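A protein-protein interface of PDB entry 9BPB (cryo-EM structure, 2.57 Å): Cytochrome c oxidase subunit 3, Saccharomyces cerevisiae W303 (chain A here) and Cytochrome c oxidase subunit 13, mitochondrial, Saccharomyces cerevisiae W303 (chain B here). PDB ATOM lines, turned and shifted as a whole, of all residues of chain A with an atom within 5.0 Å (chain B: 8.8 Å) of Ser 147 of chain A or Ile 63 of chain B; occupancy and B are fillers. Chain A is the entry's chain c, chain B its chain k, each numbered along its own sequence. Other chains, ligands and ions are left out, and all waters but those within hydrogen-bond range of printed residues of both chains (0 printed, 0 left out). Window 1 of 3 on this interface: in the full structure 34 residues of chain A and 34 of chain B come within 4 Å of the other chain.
The backbone carbonyl oxygen (O) of Ile 143 of chain A lies within hydrogen-bond range of the side-chain hydroxyl (OG) of Ser 147 of chain A, at 2.9 Å.
OG of Ser 147 of chain A is in hydrogen-bond range of O of Ile 144 of chain A.
The side-chain hydroxyl (OG) of Ser 55 of chain B sits at hydrogen-bond distance from the backbone carbonyl oxygen (O) of Trp 51 of chain B (2.8 Å).
The backbone carbonyl oxygen (O) of Ser 55 of chain B lies within hydrogen-bond range of the backbone NH (N) of Leu 60 of chain B, at 2.9 Å.
OG1 of Thr 70 of chain B sits at hydrogen-bond distance from O of Thr 66 of chain B (2.9 Å).
Hydrophobic or aromatic side chains of chain A within 4 Å of the printed part of chain B: Leu 140 and Ile 143.
Of the 18 printed residues of chain B, 4 touch a printed residue of chain A.
Printed residues of chain B that touch a printed residue of chain A: Ser 55, Ala 62, Ile 63 and Thr 66.
Along chain B the printed residues that touch a printed residue of chain A span positions 55 to 66.
Among the printed residues, 5 pairs touch across the chains.
Among the printed residues, no Asp or Glu carboxylate lies within 4 Å of a Lys or Arg side-chain nitrogen of the other chain.
Among the printed residues, merely in contact across the chains: Leu 140 of chain A with Thr 66 of chain B, Ile 143 of chain A with Ala 62 of chain B, Ile 143 of chain A with Ile 63 of chain B, Ser 147 of chain A with Ile 63 of chain B and Ala 150 of chain A with Ser 55 of chain B.
Ser 147 of chain A touches just one residue of chain B: Ile 63 (3.7 Å).
Of the printed residues of chain A, Ile 63 of chain B touches Ile 143 (3.8 Å) and Ser 147 (3.7 Å).
Of the printed residues of chain A, Ala 62 of chain B touches Ile 143.
Printed residues of chain B within 4 Å of Leu 140 of chain A: Thr 66 (3.8 Å).
Ala 59 of chain B touches none of the printed residues of chain A.
The nearest residue of chain B that does not touch Ser 147 of chain A is Ala 59 of chain B (4.04 Å).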
ATOM      1  N   LEU A 140      19.531  -2.061 -19.768  1.00  0.00           N
ATOM      2  CA  LEU A 140      20.494  -2.958 -20.397  1.00  0.00           C
ATOM      3  C   LEU A 140      21.569  -2.169 -21.132  1.00  0.00           C
ATOM      4  O   LEU A 140      22.745  -2.549 -21.126  1.00  0.00           O
ATOM      5  CB  LEU A 140      19.771  -3.916 -21.342  1.00  0.00           C
ATOM      6  CG  LEU A 140      20.611  -4.900 -22.159  1.00  0.00           C
ATOM      7  CD1 LEU A 140      21.450  -5.777 -21.246  1.00  0.00           C
ATOM      8  CD2 LEU A 140      19.713  -5.749 -23.043  1.00  0.00           C
ATOM      9  N   ILE A 143      24.161  -0.721 -18.438  1.00  0.00           N
ATOM     10  CA  ILE A 143      25.160  -1.680 -17.981  1.00  0.00           C
ATOM     11  C   ILE A 143      26.157  -1.981 -19.096  1.00  0.00           C
ATOM     12  O   ILE A 143      27.350  -2.187 -18.844  1.00  0.00           O
ATOM     13  CB  ILE A 143      24.472  -2.959 -17.473  1.00  0.00           C
ATOM     14  CG1 ILE A 143      23.493  -2.625 -16.348  1.00  0.00           C
ATOM     15  CG2 ILE A 143      25.499  -3.964 -16.987  1.00  0.00           C
ATOM     16  CD1 ILE A 143      24.121  -1.879 -15.196  1.00  0.00           C
ATOM     17  N   ILE A 144      25.682  -2.015 -20.341  1.00  0.00           N
ATOM     18  CA  ILE A 144      26.559  -2.298 -21.474  1.00  0.00           C
ATOM     19  C   ILE A 144      27.593  -1.191 -21.643  1.00  0.00           C
ATOM     20  O   ILE A 144      28.778  -1.460 -21.870  1.00  0.00           O
ATOM     21  CB  ILE A 144      25.723  -2.496 -22.751  1.00  0.00           C
ATOM     22  CG1 ILE A 144      25.123  -3.904 -22.774  1.00  0.00           C
ATOM     23  CG2 ILE A 144      26.562  -2.251 -23.988  1.00  0.00           C
ATOM     24  CD1 ILE A 144      24.071  -4.099 -23.836  1.00  0.00           C
ATOM     25  N   LEU A 145      27.165   0.069 -21.529  1.00  0.00           N
ATOM     26  CA  LEU A 145      28.084   1.181 -21.748  1.00  0.00           C
ATOM     27  C   LEU A 145      29.121   1.282 -20.634  1.00  0.00           C
ATOM     28  O   LEU A 145      30.284   1.612 -20.893  1.00  0.00           O
ATOM     29  CB  LEU A 145      27.308   2.490 -21.875  1.00  0.00           C
ATOM     30  CG  LEU A 145      27.005   2.952 -23.300  1.00  0.00           C
ATOM     31  CD1 LEU A 145      26.344   4.315 -23.290  1.00  0.00           C
ATOM     32  CD2 LEU A 145      28.269   2.974 -24.140  1.00  0.00           C
ATOM     33  N   LEU A 146      28.719   1.017 -19.389  1.00  0.00           N
ATOM     34  CA  LEU A 146      29.681   1.022 -18.291  1.00  0.00           C
ATOM     35  C   LEU A 146      30.723  -0.072 -18.466  1.00  0.00           C
ATOM     36  O   LEU A 146      31.913   0.148 -18.212  1.00  0.00           O
ATOM     37  CB  LEU A 146      28.964   0.867 -16.952  1.00  0.00           C
ATOM     38  CG  LEU A 146      28.635   2.154 -16.192  1.00  0.00           C
ATOM     39  CD1 LEU A 146      27.561   2.952 -16.905  1.00  0.00           C
ATOM     40  CD2 LEU A 146      28.210   1.832 -14.769  1.00  0.00           C
ATOM     41  N   SER A 147      30.296  -1.259 -18.902  1.00  0.00           N
ATOM     42  CA  SER A 147      31.239  -2.350 -19.118  1.00  0.00           C
ATOM     43  C   SER A 147      32.195  -2.054 -20.266  1.00  0.00           C
ATOM     44  O   SER A 147      33.300  -2.604 -20.305  1.00  0.00           O
ATOM     45  CB  SER A 147      30.483  -3.653 -19.374  1.00  0.00           C
ATOM     46  OG  SER A 147      29.477  -3.472 -20.355  1.00  0.00           O
ATOM     47  N   SER A 148      31.793  -1.193 -21.206  1.00  0.00           N
ATOM     48  CA  SER A 148      32.700  -0.797 -22.277  1.00  0.00           C
ATOM     49  C   SER A 148      33.868   0.016 -21.735  1.00  0.00           C
ATOM     50  O   SER A 148      34.999  -0.119 -22.214  1.00  0.00           O
ATOM     51  CB  SER A 148      31.946  -0.005 -23.344  1.00  0.00           C
ATOM     52  OG  SER A 148      30.743  -0.655 -23.707  1.00  0.00           O
ATOM     53  N   GLY A 149      33.613   0.869 -20.743  1.00  0.00           N
ATOM     54  CA  GLY A 149      34.681   1.641 -20.137  1.00  0.00           C
ATOM     55  C   GLY A 149      35.634   0.815 -19.301  1.00  0.00           C
ATOM     56  O   GLY A 149      36.774   1.234 -19.085  1.00  0.00           O
ATOM     57  N   ALA A 150      35.192  -0.349 -18.828  1.00  0.00           N
ATOM     58  CA  ALA A 150      36.041  -1.240 -18.055  1.00  0.00           C
ATOM     59  C   ALA A 150      36.895  -2.155 -18.922  1.00  0.00           C
ATOM     60  O   ALA A 150      37.984  -2.548 -18.491  1.00  0.00           O
ATOM     61  CB  ALA A 150      35.192  -2.092 -17.105  1.00  0.00           C
ATOM     62  N   THR A 151      36.437  -2.498 -20.128  1.00  0.00           N
ATOM     63  CA  THR A 151      37.190  -3.380 -21.007  1.00  0.00           C
ATOM     64  C   THR A 151      38.112  -2.643 -21.963  1.00  0.00           C
ATOM     65  O   THR A 151      39.048  -3.255 -22.486  1.00  0.00           O
ATOM     66  CB  THR A 151      36.243  -4.269 -21.823  1.00  0.00           C
ATOM     67  OG1 THR A 151      37.011  -5.150 -22.650  1.00  0.00           O
ATOM     68  CG2 THR A 151      35.341  -3.424 -22.702  1.00  0.00           C
ATOM     69  N   LEU A 177      30.645  -4.820 -28.144  1.00  0.00           N
ATOM     70  CA  LEU A 177      29.805  -4.335 -27.060  1.00  0.00           C
ATOM     71  C   LEU A 177      29.238  -2.954 -27.358  1.00  0.00           C
ATOM     72  O   LEU A 177      28.252  -2.552 -26.732  1.00  0.00           O
ATOM     73  CB  LEU A 177      30.607  -4.318 -25.755  1.00  0.00           C
ATOM     74  CG  LEU A 177      29.909  -4.037 -24.429  1.00  0.00           C
ATOM     75  CD1 LEU A 177      28.899  -5.132 -24.139  1.00  0.00           C
ATOM     76  CD2 LEU A 177      30.936  -3.953 -23.317  1.00  0.00           C
ATOM     77  N   TRP B  51      41.858  -4.664 -13.496  1.00  0.00           N
ATOM     78  CA  TRP B  51      40.664  -4.380 -14.282  1.00  0.00           C
ATOM     79  C   TRP B  51      40.088  -5.640 -14.912  1.00  0.00           C
ATOM     80  O   TRP B  51      38.881  -5.704 -15.173  1.00  0.00           O
ATOM     81  CB  TRP B  51      40.977  -3.336 -15.352  1.00  0.00           C
ATOM     82  CG  TRP B  51      40.946  -1.941 -14.817  1.00  0.00           C
ATOM     83  CD1 TRP B  51      42.019  -1.157 -14.511  1.00  0.00           C
ATOM     84  CD2 TRP B  51      39.781  -1.169 -14.504  1.00  0.00           C
ATOM     85  NE1 TRP B  51      41.593   0.059 -14.032  1.00  0.00           N
ATOM     86  CE2 TRP B  51      40.224   0.075 -14.019  1.00  0.00           C
ATOM     87  CE3 TRP B  51      38.407  -1.410 -14.589  1.00  0.00           C
ATOM     88  CZ2 TRP B  51      39.342   1.078 -13.620  1.00  0.00           C
ATOM     89  CZ3 TRP B  51      37.535  -0.414 -14.195  1.00  0.00           C
ATOM     90  CH2 TRP B  51      38.004   0.813 -13.717  1.00  0.00           C
ATOM     91  N   ILE B  54      37.948  -7.014 -12.191  1.00  0.00           N
ATOM     92  CA  ILE B  54      36.700  -6.263 -12.119  1.00  0.00           C
ATOM     93  C   ILE B  54      35.762  -6.672 -13.246  1.00  0.00           C
ATOM     94  O   ILE B  54      34.554  -6.835 -13.039  1.00  0.00           O
ATOM     95  CB  ILE B  54      36.984  -4.750 -12.143  1.00  0.00           C
ATOM     96  CG1 ILE B  54      37.796  -4.339 -10.914  1.00  0.00           C
ATOM     97  CG2 ILE B  54      35.686  -3.961 -12.209  1.00  0.00           C
ATOM     98  CD1 ILE B  54      38.320  -2.924 -10.977  1.00  0.00           C
ATOM     99  N   SER B  55      36.299  -6.846 -14.456  1.00  0.00           N
ATOM    100  CA  SER B  55      35.459  -7.175 -15.604  1.00  0.00           C
ATOM    101  C   SER B  55      34.754  -8.513 -15.410  1.00  0.00           C
ATOM    102  O   SER B  55      33.536  -8.619 -15.594  1.00  0.00           O
ATOM    103  CB  SER B  55      36.303  -7.195 -16.879  1.00  0.00           C
ATOM    104  OG  SER B  55      36.887  -5.927 -17.126  1.00  0.00           O
ATOM    105  N   VAL B  56      35.507  -9.548 -15.039  1.00  0.00           N
ATOM    106  CA  VAL B  56      34.932 -10.885 -14.935  1.00  0.00           C
ATOM    107  C   VAL B  56      33.998 -10.986 -13.734  1.00  0.00           C
ATOM    108  O   VAL B  56      32.940 -11.622 -13.809  1.00  0.00           O
ATOM    109  CB  VAL B  56      36.049 -11.943 -14.876  1.00  0.00           C
ATOM    110  CG1 VAL B  56      35.454 -13.339 -14.889  1.00  0.00           C
ATOM    111  CG2 VAL B  56      37.006 -11.763 -16.041  1.00  0.00           C
ATOM    112  N   VAL B  58      32.504  -8.461 -11.850  1.00  0.00           N
ATOM    113  CA  VAL B  58      31.493  -7.426 -11.667  1.00  0.00           C
ATOM    114  C   VAL B  58      30.695  -7.190 -12.945  1.00  0.00           C
ATOM    115  O   VAL B  58      29.464  -7.275 -12.946  1.00  0.00           O
ATOM    116  CB  VAL B  58      32.122  -6.103 -11.169  1.00  0.00           C
ATOM    117  CG1 VAL B  58      31.034  -5.122 -10.768  1.00  0.00           C
ATOM    118  CG2 VAL B  58      33.069  -6.362 -10.009  1.00  0.00           C
ATOM    119  N   ALA B  59      31.386  -6.890 -14.047  1.00  0.00           N
ATOM    120  CA  ALA B  59      30.695  -6.540 -15.286  1.00  0.00           C
ATOM    121  C   ALA B  59      29.963  -7.740 -15.873  1.00  0.00           C
ATOM    122  O   ALA B  59      28.788  -7.639 -16.247  1.00  0.00           O
ATOM    123  CB  ALA B  59      31.691  -5.967 -16.295  1.00  0.00           C
ATOM    124  N   LEU B  60      30.643  -8.882 -15.971  1.00  0.00           N
ATOM    125  CA  LEU B  60      30.022 -10.066 -16.562  1.00  0.00           C
ATOM    126  C   LEU B  60      28.796 -10.541 -15.788  1.00  0.00           C
ATOM    127  O   LEU B  60      27.757 -10.791 -16.422  1.00  0.00           O
ATOM    128  CB  LEU B  60      31.073 -11.174 -16.711  1.00  0.00           C
ATOM    129  CG  LEU B  60      30.746 -12.397 -17.571  1.00  0.00           C
ATOM    130  CD1 LEU B  60      32.009 -12.923 -18.230  1.00  0.00           C
ATOM    131  CD2 LEU B  60      30.092 -13.494 -16.747  1.00  0.00           C
ATOM    132  N   PRO B  61      28.833 -10.703 -14.458  1.00  0.00           N
ATOM    133  CA  PRO B  61      27.595 -11.073 -13.752  1.00  0.00           C
ATOM    134  C   PRO B  61      26.489 -10.043 -13.889  1.00  0.00           C
ATOM    135  O   PRO B  61      25.312 -10.416 -13.948  1.00  0.00           O
ATOM    136  CB  PRO B  61      28.054 -11.213 -12.294  1.00  0.00           C
ATOM    137  CG  PRO B  61      29.509 -11.485 -12.385  1.00  0.00           C
ATOM    138  CD  PRO B  61      29.973 -10.643 -13.527  1.00  0.00           C
ATOM    139  N   ALA B  62      26.835  -8.754 -13.936  1.00  0.00           N
ATOM    140  CA  ALA B  62      25.815  -7.715 -14.042  1.00  0.00           C
ATOM    141  C   ALA B  62      25.047  -7.830 -15.352  1.00  0.00           C
ATOM    142  O   ALA B  62      23.816  -7.718 -15.374  1.00  0.00           O
ATOM    143  CB  ALA B  62      26.458  -6.334 -13.911  1.00  0.00           C
ATOM    144  N   ILE B  63      25.760  -8.059 -16.457  1.00  0.00           N
ATOM    145  CA  ILE B  63      25.099  -8.199 -17.751  1.00  0.00           C
ATOM    146  C   ILE B  63      24.243  -9.458 -17.782  1.00  0.00           C
ATOM    147  O   ILE B  63      23.128  -9.454 -18.317  1.00  0.00           O
ATOM    148  CB  ILE B  63      26.137  -8.188 -18.886  1.00  0.00           C
ATOM    149  CG1 ILE B  63      26.969  -6.908 -18.834  1.00  0.00           C
ATOM    150  CG2 ILE B  63      25.454  -8.324 -20.236  1.00  0.00           C
ATOM    151  CD1 ILE B  63      27.993  -6.803 -19.937  1.00  0.00           C
ATOM    152  N   ALA B  64      24.744 -10.555 -17.212  1.00  0.00           N
ATOM    153  CA  ALA B  64      23.997 -11.806 -17.219  1.00  0.00           C
ATOM    154  C   ALA B  64      22.708 -11.721 -16.415  1.00  0.00           C
ATOM    155  O   ALA B  64      21.713 -12.338 -16.804  1.00  0.00           O
ATOM    156  CB  ALA B  64      24.867 -12.943 -16.683  1.00  0.00           C
ATOM    157  N   LEU B  65      22.699 -10.974 -15.310  1.00  0.00           N
ATOM    158  CA  LEU B  65      21.503 -10.844 -14.490  1.00  0.00           C
ATOM    159  C   LEU B  65      20.512  -9.816 -15.018  1.00  0.00           C
ATOM    160  O   LEU B  65      19.364  -9.800 -14.562  1.00  0.00           O
ATOM    161  CB  LEU B  65      21.877 -10.478 -13.048  1.00  0.00           C
ATOM    162  CG  LEU B  65      22.705 -11.505 -12.273  1.00  0.00           C
ATOM    163  CD1 LEU B  65      23.476 -10.831 -11.150  1.00  0.00           C
ATOM    164  CD2 LEU B  65      21.819 -12.612 -11.731  1.00  0.00           C
ATOM    165  N   THR B  66      20.918  -8.960 -15.954  1.00  0.00           N
ATOM    166  CA  THR B  66      19.994  -8.015 -16.570  1.00  0.00           C
ATOM    167  C   THR B  66      19.575  -8.426 -17.973  1.00  0.00           C
ATOM    168  O   THR B  66      18.534  -7.967 -18.453  1.00  0.00           O
ATOM    169  CB  THR B  66      20.607  -6.610 -16.616  1.00  0.00           C
ATOM    170  OG1 THR B  66      19.630  -5.679 -17.094  1.00  0.00           O
ATOM    171  CG2 THR B  66      21.807  -6.576 -17.542  1.00  0.00           C
ATOM    172  N   ALA B  67      20.360  -9.273 -18.641  1.00  0.00           N
ATOM    173  CA  ALA B  67      19.961  -9.765 -19.955  1.00  0.00           C
ATOM    174  C   ALA B  67      18.851 -10.800 -19.840  1.00  0.00           C
ATOM    175  O   ALA B  67      17.911 -10.803 -20.644  1.00  0.00           O
ATOM    176  CB  ALA B  67      21.166 -10.350 -20.690  1.00  0.00           C
ATOM    177  N   VAL B  68      18.941 -11.690 -18.847  1.00  0.00           N
ATOM    178  CA  VAL B  68      17.892 -12.685 -18.653  1.00  0.00           C
ATOM    179  C   VAL B  68      16.596 -12.017 -18.214  1.00  0.00           C
ATOM    180  O   VAL B  68      15.504 -12.506 -18.521  1.00  0.00           O
ATOM    181  CB  VAL B  68      18.349 -13.762 -17.650  1.00  0.00           C
ATOM    182  CG1 VAL B  68      19.576 -14.485 -18.176  1.00  0.00           C
ATOM    183  CG2 VAL B  68      18.634 -13.147 -16.288  1.00  0.00           C
ATOM    184  N   ASN B  69      16.688 -10.900 -17.490  1.00  0.00           N
ATOM    185  CA  ASN B  69      15.487 -10.166 -17.114  1.00  0.00           C
ATOM    186  C   ASN B  69      14.881  -9.449 -18.312  1.00  0.00           C
ATOM    187  O   ASN B  69      13.662  -9.486 -18.513  1.00  0.00           O
ATOM    188  CB  ASN B  69      15.808  -9.173 -15.998  1.00  0.00           C
ATOM    189  CG  ASN B  69      14.565  -8.651 -15.310  1.00  0.00           C
ATOM    190  OD1 ASN B  69      14.000  -9.311 -14.440  1.00  0.00           O
ATOM    191  ND2 ASN B  69      14.132  -7.457 -15.698  1.00  0.00           N
ATOM    192  N   THR B  70      15.717  -8.794 -19.122  1.00  0.00           N
ATOM    193  CA  THR B  70      15.213  -8.080 -20.291  1.00  0.00           C
ATOM    194  C   THR B  70      14.637  -9.045 -21.321  1.00  0.00           C
ATOM    195  O   THR B  70      13.651  -8.725 -21.993  1.00  0.00           O
ATOM    196  CB  THR B  70      16.332  -7.236 -20.904  1.00  0.00           C
ATOM    197  OG1 THR B  70      16.783  -6.274 -19.943  1.00  0.00           O
ATOM    198  CG2 THR B  70      15.840  -6.505 -22.143  1.00  0.00           C
ATOM    199  N   TYR B  71      15.235 -10.232 -21.448  1.00  0.00           N
ATOM    200  CA  TYR B  71      14.732 -11.229 -22.387  1.00  0.00           C
ATOM    201  C   TYR B  71      13.298 -11.623 -22.058  1.00  0.00           C
ATOM    202  O   TYR B  71      12.455 -11.757 -22.952  1.00  0.00           O
ATOM    203  CB  TYR B  71      15.642 -12.457 -22.379  1.00  0.00           C
ATOM    204  CG  TYR B  71      15.227 -13.553 -23.336  1.00  0.00           C
ATOM    205  CD1 TYR B  71      15.665 -13.553 -24.653  1.00  0.00           C
ATOM    206  CD2 TYR B  71      14.398 -14.587 -22.921  1.00  0.00           C
ATOM    207  CE1 TYR B  71      15.289 -14.554 -25.531  1.00  0.00           C
ATOM    208  CE2 TYR B  71      14.015 -15.591 -23.791  1.00  0.00           C
ATOM    209  CZ  TYR B  71      14.464 -15.569 -25.093  1.00  0.00           C
ATOM    210  OH  TYR B  71      14.085 -16.567 -25.962  1.00  0.00           O
